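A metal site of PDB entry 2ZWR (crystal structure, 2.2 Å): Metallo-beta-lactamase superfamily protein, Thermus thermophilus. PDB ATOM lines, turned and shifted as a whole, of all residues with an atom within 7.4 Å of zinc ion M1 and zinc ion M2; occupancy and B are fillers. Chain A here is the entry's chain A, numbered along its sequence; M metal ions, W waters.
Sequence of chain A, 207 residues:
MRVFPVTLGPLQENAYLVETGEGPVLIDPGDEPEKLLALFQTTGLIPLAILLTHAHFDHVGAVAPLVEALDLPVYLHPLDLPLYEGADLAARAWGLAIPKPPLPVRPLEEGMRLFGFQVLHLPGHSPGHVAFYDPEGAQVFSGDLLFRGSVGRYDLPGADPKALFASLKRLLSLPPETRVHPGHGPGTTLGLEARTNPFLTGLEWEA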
ATOM      1  N   LEU A  11       7.081  24.627  -8.266  1.00  0.00           N
ATOM      2  CA  LEU A  11       6.621  24.397  -6.910  1.00  0.00           C
ATOM      3  C   LEU A  11       7.646  24.895  -5.890  1.00  0.00           C
ATOM      4  O   LEU A  11       7.503  24.693  -4.690  1.00  0.00           O
ATOM      5  CB  LEU A  11       6.251  22.921  -6.666  1.00  0.00           C
ATOM      6  CG  LEU A  11       4.858  22.392  -7.094  1.00  0.00           C
ATOM      7  CD1 LEU A  11       3.720  23.297  -6.588  1.00  0.00           C
ATOM      8  CD2 LEU A  11       4.721  22.206  -8.602  1.00  0.00           C
ATOM      9  N   GLN A  12       8.690  25.569  -6.388  1.00  0.00           N
ATOM     10  CA  GLN A  12       9.679  26.239  -5.554  1.00  0.00           C
ATOM     11  C   GLN A  12      10.219  25.324  -4.443  1.00  0.00           C
ATOM     12  O   GLN A  12      10.077  25.597  -3.238  1.00  0.00           O
ATOM     13  CB  GLN A  12       9.096  27.543  -5.017  1.00  0.00           C
ATOM     14  CG  GLN A  12       8.920  28.603  -6.107  1.00  0.00           C
ATOM     15  CD  GLN A  12       8.293  29.886  -5.617  1.00  0.00           C
ATOM     16  OE1 GLN A  12       7.424  29.882  -4.738  1.00  0.00           O
ATOM     17  NE2 GLN A  12       8.727  30.999  -6.197  1.00  0.00           N
ATOM     18  N   GLU A  13      10.814  24.220  -4.870  1.00  0.00           N
ATOM     19  CA  GLU A  13      11.316  23.191  -3.980  1.00  0.00           C
ATOM     20  C   GLU A  13      12.790  23.456  -3.714  1.00  0.00           C
ATOM     21  O   GLU A  13      13.492  23.946  -4.607  1.00  0.00           O
ATOM     22  CB  GLU A  13      11.086  21.817  -4.619  1.00  0.00           C
ATOM     23  CG  GLU A  13      11.692  20.613  -3.873  1.00  0.00           C
ATOM     24  CD  GLU A  13      13.071  20.222  -4.391  1.00  0.00           C
ATOM     25  OE1 GLU A  13      13.545  20.790  -5.390  1.00  0.00           O
ATOM     26  OE2 GLU A  13      13.699  19.337  -3.772  1.00  0.00           O
ATOM     27  N   ASN A  14      13.261  23.155  -2.501  1.00  0.00           N
ATOM     28  CA  ASN A  14      14.676  23.335  -2.152  1.00  0.00           C
ATOM     29  C   ASN A  14      15.534  22.053  -2.265  1.00  0.00           C
ATOM     30  O   ASN A  14      15.303  21.064  -1.534  1.00  0.00           O
ATOM     31  CB  ASN A  14      14.841  23.895  -0.719  1.00  0.00           C
ATOM     32  CG  ASN A  14      14.026  25.170  -0.461  1.00  0.00           C
ATOM     33  OD1 ASN A  14      13.511  25.361   0.645  1.00  0.00           O
ATOM     34  ND2 ASN A  14      13.929  26.048  -1.455  1.00  0.00           N
ATOM     35  N   ASP A  28      17.366  15.914  -2.854  1.00  0.00           N
ATOM     36  CA  ASP A  28      16.119  16.315  -3.552  1.00  0.00           C
ATOM     37  C   ASP A  28      16.309  17.208  -4.802  1.00  0.00           C
ATOM     38  O   ASP A  28      15.808  18.349  -4.833  1.00  0.00           O
ATOM     39  CB  ASP A  28      15.131  17.000  -2.583  1.00  0.00           C
ATOM     40  CG  ASP A  28      14.648  16.097  -1.462  1.00  0.00           C
ATOM     41  OD1 ASP A  28      15.019  14.899  -1.412  1.00  0.00           O
ATOM     42  OD2 ASP A  28      13.884  16.602  -0.610  1.00  0.00           O
ATOM     43  N   THR A  53      14.530  12.788   0.463  1.00  0.00           N
ATOM     44  CA  THR A  53      13.672  12.847   1.645  1.00  0.00           C
ATOM     45  C   THR A  53      12.367  12.148   1.339  1.00  0.00           C
ATOM     46  O   THR A  53      11.847  11.418   2.184  1.00  0.00           O
ATOM     47  CB  THR A  53      13.358  14.301   2.124  1.00  0.00           C
ATOM     48  OG1 THR A  53      12.586  14.984   1.113  1.00  0.00           O
ATOM     49  CG2 THR A  53      14.642  15.077   2.471  1.00  0.00           C
ATOM     50  N   HIS A  54      11.866  12.349   0.123  1.00  0.00           N
ATOM     51  CA  HIS A  54      10.682  11.618  -0.367  1.00  0.00           C
ATOM     52  C   HIS A  54      10.570  11.761  -1.890  1.00  0.00           C
ATOM     53  O   HIS A  54      11.404  12.420  -2.508  1.00  0.00           O
ATOM     54  CB  HIS A  54       9.416  12.058   0.378  1.00  0.00           C
ATOM     55  CG  HIS A  54       8.988  13.483   0.091  1.00  0.00           C
ATOM     56  ND1 HIS A  54       9.766  14.575   0.399  1.00  0.00           N
ATOM     57  CD2 HIS A  54       7.845  13.980  -0.431  1.00  0.00           C
ATOM     58  CE1 HIS A  54       9.133  15.680   0.064  1.00  0.00           C
ATOM     59  NE2 HIS A  54       7.961  15.345  -0.442  1.00  0.00           N
ATOM     60  N   ALA A  55       9.540  11.146  -2.476  1.00  0.00           N
ATOM     61  CA  ALA A  55       9.427  11.026  -3.942  1.00  0.00           C
ATOM     62  C   ALA A  55       8.207  11.696  -4.565  1.00  0.00           C
ATOM     63  O   ALA A  55       7.771  11.282  -5.643  1.00  0.00           O
ATOM     64  CB  ALA A  55       9.508   9.576  -4.371  1.00  0.00           C
ATOM     65  N   HIS A  56       7.660  12.727  -3.934  1.00  0.00           N
ATOM     66  CA  HIS A  56       6.780  13.622  -4.676  1.00  0.00           C
ATOM     67  C   HIS A  56       7.556  14.211  -5.868  1.00  0.00           C
ATOM     68  O   HIS A  56       8.774  14.457  -5.784  1.00  0.00           O
ATOM     69  CB  HIS A  56       6.230  14.746  -3.806  1.00  0.00           C
ATOM     70  CG  HIS A  56       5.215  14.281  -2.835  1.00  0.00           C
ATOM     71  ND1 HIS A  56       5.000  14.919  -1.629  1.00  0.00           N
ATOM     72  CD2 HIS A  56       4.353  13.232  -2.873  1.00  0.00           C
ATOM     73  CE1 HIS A  56       4.043  14.283  -0.963  1.00  0.00           C
ATOM     74  NE2 HIS A  56       3.631  13.261  -1.698  1.00  0.00           N
ATOM     75  N   PHE A  57       6.837  14.400  -6.974  1.00  0.00           N
ATOM     76  CA  PHE A  57       7.449  14.819  -8.237  1.00  0.00           C
ATOM     77  C   PHE A  57       8.281  16.099  -8.166  1.00  0.00           C
ATOM     78  O   PHE A  57       9.240  16.243  -8.936  1.00  0.00           O
ATOM     79  CB  PHE A  57       6.399  14.896  -9.365  1.00  0.00           C
ATOM     80  CG  PHE A  57       5.444  16.073  -9.277  1.00  0.00           C
ATOM     81  CD1 PHE A  57       4.146  15.888  -8.818  1.00  0.00           C
ATOM     82  CD2 PHE A  57       5.818  17.350  -9.713  1.00  0.00           C
ATOM     83  CE1 PHE A  57       3.235  16.960  -8.751  1.00  0.00           C
ATOM     84  CE2 PHE A  57       4.924  18.432  -9.658  1.00  0.00           C
ATOM     85  CZ  PHE A  57       3.624  18.232  -9.171  1.00  0.00           C
ATOM     86  N   ASP A  58       7.929  17.014  -7.264  1.00  0.00           N
ATOM     87  CA  ASP A  58       8.693  18.259  -7.118  1.00  0.00           C
ATOM     88  C   ASP A  58      10.065  18.064  -6.458  1.00  0.00           C
ATOM     89  O   ASP A  58      10.870  18.988  -6.388  1.00  0.00           O
ATOM     90  CB  ASP A  58       7.873  19.357  -6.401  1.00  0.00           C
ATOM     91  CG  ASP A  58       7.383  18.932  -5.022  1.00  0.00           C
ATOM     92  OD1 ASP A  58       6.815  17.821  -4.886  1.00  0.00           O
ATOM     93  OD2 ASP A  58       7.559  19.701  -4.062  1.00  0.00           O
ATOM     94  N   HIS A  59      10.331  16.841  -5.998  1.00  0.00           N
ATOM     95  CA  HIS A  59      11.607  16.517  -5.364  1.00  0.00           C
ATOM     96  C   HIS A  59      12.509  15.629  -6.237  1.00  0.00           C
ATOM     97  O   HIS A  59      13.672  15.414  -5.905  1.00  0.00           O
ATOM     98  CB  HIS A  59      11.378  15.909  -3.970  1.00  0.00           C
ATOM     99  CG  HIS A  59      10.801  16.886  -2.991  1.00  0.00           C
ATOM    100  ND1 HIS A  59      11.544  17.490  -2.006  1.00  0.00           N
ATOM    101  CD2 HIS A  59       9.556  17.412  -2.900  1.00  0.00           C
ATOM    102  CE1 HIS A  59      10.789  18.334  -1.325  1.00  0.00           C
ATOM    103  NE2 HIS A  59       9.580  18.317  -1.856  1.00  0.00           N
ATOM    104  N   HIS A 125       3.606  12.934   5.506  1.00  0.00           N
ATOM    105  CA  HIS A 125       3.497  13.711   4.260  1.00  0.00           C
ATOM    106  C   HIS A 125       3.553  12.728   3.074  1.00  0.00           C
ATOM    107  O   HIS A 125       2.856  12.908   2.062  1.00  0.00           O
ATOM    108  CB  HIS A 125       4.595  14.773   4.196  1.00  0.00           C
ATOM    109  CG  HIS A 125       4.602  15.587   2.938  1.00  0.00           C
ATOM    110  ND1 HIS A 125       3.741  16.630   2.714  1.00  0.00           N
ATOM    111  CD2 HIS A 125       5.398  15.524   1.841  1.00  0.00           C
ATOM    112  CE1 HIS A 125       3.979  17.171   1.537  1.00  0.00           C
ATOM    113  NE2 HIS A 125       4.992  16.515   0.983  1.00  0.00           N
ATOM    114  N   SER A 126       4.363  11.679   3.220  1.00  0.00           N
ATOM    115  CA  SER A 126       4.379  10.538   2.310  1.00  0.00           C
ATOM    116  C   SER A 126       4.864   9.313   3.101  1.00  0.00           C
ATOM    117  O   SER A 126       5.491   9.466   4.133  1.00  0.00           O
ATOM    118  CB  SER A 126       5.277  10.807   1.080  1.00  0.00           C
ATOM    119  OG  SER A 126       6.643  10.806   1.441  1.00  0.00           O
ATOM    120  N   HIS A 129       8.727   9.031   3.713  1.00  0.00           N
ATOM    121  CA  HIS A 129       9.349  10.330   3.970  1.00  0.00           C
ATOM    122  C   HIS A 129      10.386  10.177   5.081  1.00  0.00           C
ATOM    123  O   HIS A 129      10.064   9.691   6.177  1.00  0.00           O
ATOM    124  CB  HIS A 129       8.299  11.380   4.356  1.00  0.00           C
ATOM    125  CG  HIS A 129       8.794  12.794   4.270  1.00  0.00           C
ATOM    126  ND1 HIS A 129       9.797  13.281   5.081  1.00  0.00           N
ATOM    127  CD2 HIS A 129       8.433  13.819   3.456  1.00  0.00           C
ATOM    128  CE1 HIS A 129      10.036  14.549   4.768  1.00  0.00           C
ATOM    129  NE2 HIS A 129       9.218  14.896   3.797  1.00  0.00           N
ATOM    130  N   GLY A 143      12.948  17.611   4.640  1.00  0.00           N
ATOM    131  CA  GLY A 143      11.998  17.633   3.535  1.00  0.00           C
ATOM    132  C   GLY A 143      10.756  18.453   3.820  1.00  0.00           C
ATOM    133  O   GLY A 143      10.841  19.604   4.259  1.00  0.00           O
ATOM    134  N   ASP A 144       9.599  17.856   3.573  1.00  0.00           N
ATOM    135  CA  ASP A 144       8.343  18.580   3.725  1.00  0.00           C
ATOM    136  C   ASP A 144       7.637  18.269   5.043  1.00  0.00           C
ATOM    137  O   ASP A 144       6.417  18.345   5.118  1.00  0.00           O
ATOM    138  CB  ASP A 144       7.412  18.297   2.544  1.00  0.00           C
ATOM    139  CG  ASP A 144       7.964  18.803   1.220  1.00  0.00           C
ATOM    140  OD1 ASP A 144       9.073  19.405   1.218  1.00  0.00           O
ATOM    141  OD2 ASP A 144       7.289  18.587   0.175  1.00  0.00           O
ATOM    142  N   LEU A 145       8.400  17.915   6.086  1.00  0.00           N
ATOM    143  CA  LEU A 145       7.812  17.716   7.429  1.00  0.00           C
ATOM    144  C   LEU A 145       7.438  19.073   8.060  1.00  0.00           C
ATOM    145  O   LEU A 145       6.279  19.328   8.397  1.00  0.00           O
ATOM    146  CB  LEU A 145       8.793  16.985   8.351  1.00  0.00           C
ATOM    147  CG  LEU A 145       8.705  15.455   8.445  1.00  0.00           C
ATOM    148  N   PHE A 147       8.017  23.380   8.030  1.00  0.00           N
ATOM    149  CA  PHE A 147       8.391  24.617   7.363  1.00  0.00           C
ATOM    150  C   PHE A 147       8.548  25.750   8.374  1.00  0.00           C
ATOM    151  O   PHE A 147       8.239  25.587   9.548  1.00  0.00           O
ATOM    152  CB  PHE A 147       7.366  25.011   6.288  1.00  0.00           C
ATOM    153  CG  PHE A 147       7.145  23.935   5.246  1.00  0.00           C
ATOM    154  CD1 PHE A 147       8.235  23.266   4.669  1.00  0.00           C
ATOM    155  CD2 PHE A 147       5.867  23.584   4.848  1.00  0.00           C
ATOM    156  CE1 PHE A 147       8.044  22.264   3.702  1.00  0.00           C
ATOM    157  CE2 PHE A 147       5.658  22.594   3.894  1.00  0.00           C
ATOM    158  CZ  PHE A 147       6.765  21.935   3.305  1.00  0.00           C
ATOM    159  N   GLY A 152       4.150  20.225   6.437  1.00  0.00           N
ATOM    160  CA  GLY A 152       3.841  19.609   5.145  1.00  0.00           C
ATOM    161  C   GLY A 152       2.359  19.368   4.942  1.00  0.00           C
ATOM    162  O   GLY A 152       1.639  19.052   5.890  1.00  0.00           O
ATOM    163  N   ARG A 153       1.901  19.545   3.705  1.00  0.00           N
ATOM    164  CA  ARG A 153       0.546  19.151   3.307  1.00  0.00           C
ATOM    165  C   ARG A 153       0.287  17.698   3.693  1.00  0.00           C
ATOM    166  O   ARG A 153       1.181  16.843   3.583  1.00  0.00           O
ATOM    167  CB  ARG A 153       0.337  19.329   1.800  1.00  0.00           C
ATOM    168  CG  ARG A 153       0.345  20.789   1.340  1.00  0.00           C
ATOM    169  CD  ARG A 153       0.182  20.911  -0.170  1.00  0.00           C
ATOM    170  NE  ARG A 153      -1.177  20.595  -0.608  1.00  0.00           N
ATOM    171  CZ  ARG A 153      -1.615  20.657  -1.860  1.00  0.00           C
ATOM    172  NH1 ARG A 153      -0.803  21.015  -2.841  1.00  0.00           N
ATOM    173  NH2 ARG A 153      -2.880  20.354  -2.145  1.00  0.00           N
ATOM    174  N   LEU A 156      -1.887  15.210   0.087  1.00  0.00           N
ATOM    175  CA  LEU A 156      -1.234  14.736  -1.141  1.00  0.00           C
ATOM    176  C   LEU A 156      -1.201  13.208  -1.208  1.00  0.00           C
ATOM    177  O   LEU A 156      -1.578  12.535  -0.247  1.00  0.00           O
ATOM    178  CB  LEU A 156       0.181  15.313  -1.250  1.00  0.00           C
ATOM    179  CG  LEU A 156       0.313  16.795  -1.625  1.00  0.00           C
ATOM    180  CD1 LEU A 156       1.780  17.203  -1.653  1.00  0.00           C
ATOM    181  CD2 LEU A 156      -0.365  17.072  -2.962  1.00  0.00           C
ATOM    182  N   PRO A 157      -0.804  12.648  -2.381  1.00  0.00           N
ATOM    183  CA  PRO A 157      -0.661  11.187  -2.519  1.00  0.00           C
ATOM    184  C   PRO A 157       0.243  10.561  -1.462  1.00  0.00           C
ATOM    185  O   PRO A 157       1.406  10.991  -1.269  1.00  0.00           O
ATOM    186  CB  PRO A 157      -0.069  11.028  -3.930  1.00  0.00           C
ATOM    187  CG  PRO A 157      -0.587  12.208  -4.675  1.00  0.00           C
ATOM    188  CD  PRO A 157      -0.521  13.337  -3.658  1.00  0.00           C
ATOM    189  N   GLY A 183      12.035  21.307   2.543  1.00  0.00           N
ATOM    190  CA  GLY A 183      11.784  21.142   1.112  1.00  0.00           C
ATOM    191  C   GLY A 183      11.208  22.350   0.396  1.00  0.00           C
ATOM    192  O   GLY A 183      11.273  22.424  -0.821  1.00  0.00           O
ATOM    193  N   HIS A 184      10.618  23.281   1.147  1.00  0.00           N
ATOM    194  CA  HIS A 184      10.049  24.528   0.601  1.00  0.00           C
ATOM    195  C   HIS A 184      10.218  25.676   1.589  1.00  0.00           C
ATOM    196  O   HIS A 184      10.175  25.479   2.787  1.00  0.00           O
ATOM    197  CB  HIS A 184       8.553  24.379   0.261  1.00  0.00           C
ATOM    198  CG  HIS A 184       8.249  23.186  -0.602  1.00  0.00           C
ATOM    199  ND1 HIS A 184       8.178  23.272  -1.976  1.00  0.00           N
ATOM    200  CD2 HIS A 184       8.044  21.892  -0.290  1.00  0.00           C
ATOM    201  CE1 HIS A 184       7.934  22.063  -2.474  1.00  0.00           C
ATOM    202  NE2 HIS A 184       7.849  21.212  -1.470  1.00  0.00           N
HETATM  203 ZN    ZN M   1       6.155  16.532  -0.778  1.00  0.00          ZN
HETATM  204 ZN    ZN M   2       7.698  19.270  -1.791  1.00  0.00          ZN
HETATM  205  O   HOH W   1       6.310  18.014  -2.207  1.00  0.00           O
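A ring nitrogen (NE2) of His 129 sits close to a ring nitrogen (ND1) of His 54 (3.5 Å).
ND1 of His 54 sits at hydrogen-bond distance from OG1 of Thr 53, at 2.9 Å.
The backbone carbonyl oxygen (O) of Leu 11 lies within hydrogen-bond range of a ring nitrogen (ND1) of His 184, 3.1 Å away.
The backbone carbonyl oxygen (O) of Arg 153 is in hydrogen-bond range of a ring nitrogen (ND1) of His 125, at 2.7 Å.
The backbone carbonyl oxygen (O) of Asp 144 sits close to the backbone NH (N) of Gly 152, 3.2 Å away.
A ring nitrogen (ND1) of His 184 lies within hydrogen-bond range of the backbone carbonyl oxygen (O) of Gln 12, 3.3 Å away.
NE2 of His 129 is in hydrogen-bond range of N of Asp 144, at 3.0 Å.
OE2 of Glu 13 is in hydrogen-bond range of ND1 of His 59 (3.3 Å).
Within 4 Å of zinc ion M1: His 54, His 56, His 125 and Asp 144.
Of the 25 residues printed, 4 come within 4 Å of zinc ion M2.
Zinc ion M1 is bound by water W1, 2.1 Å away.
NE2 of His 125 is bound to zinc ion M1.
ND1 of His 56 is bound to zinc ion M1 (2.2 Å).
NE2 of His 54 binds zinc ion M1 (2.2 Å).
Zinc ion M1 is bound by OD2 of Asp 144, 2.5 Å away.
Zinc ion M2 is bound by water W1 (1.9 Å), NE2 of His 184 (2.0 Å), NE2 of His 59 (2.1 Å), OD2 of Asp 144 (2.1 Å) and OD2 of Asp 58 (2.3 Å).
Zinc ion M2 has five donor atoms within binding distance.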
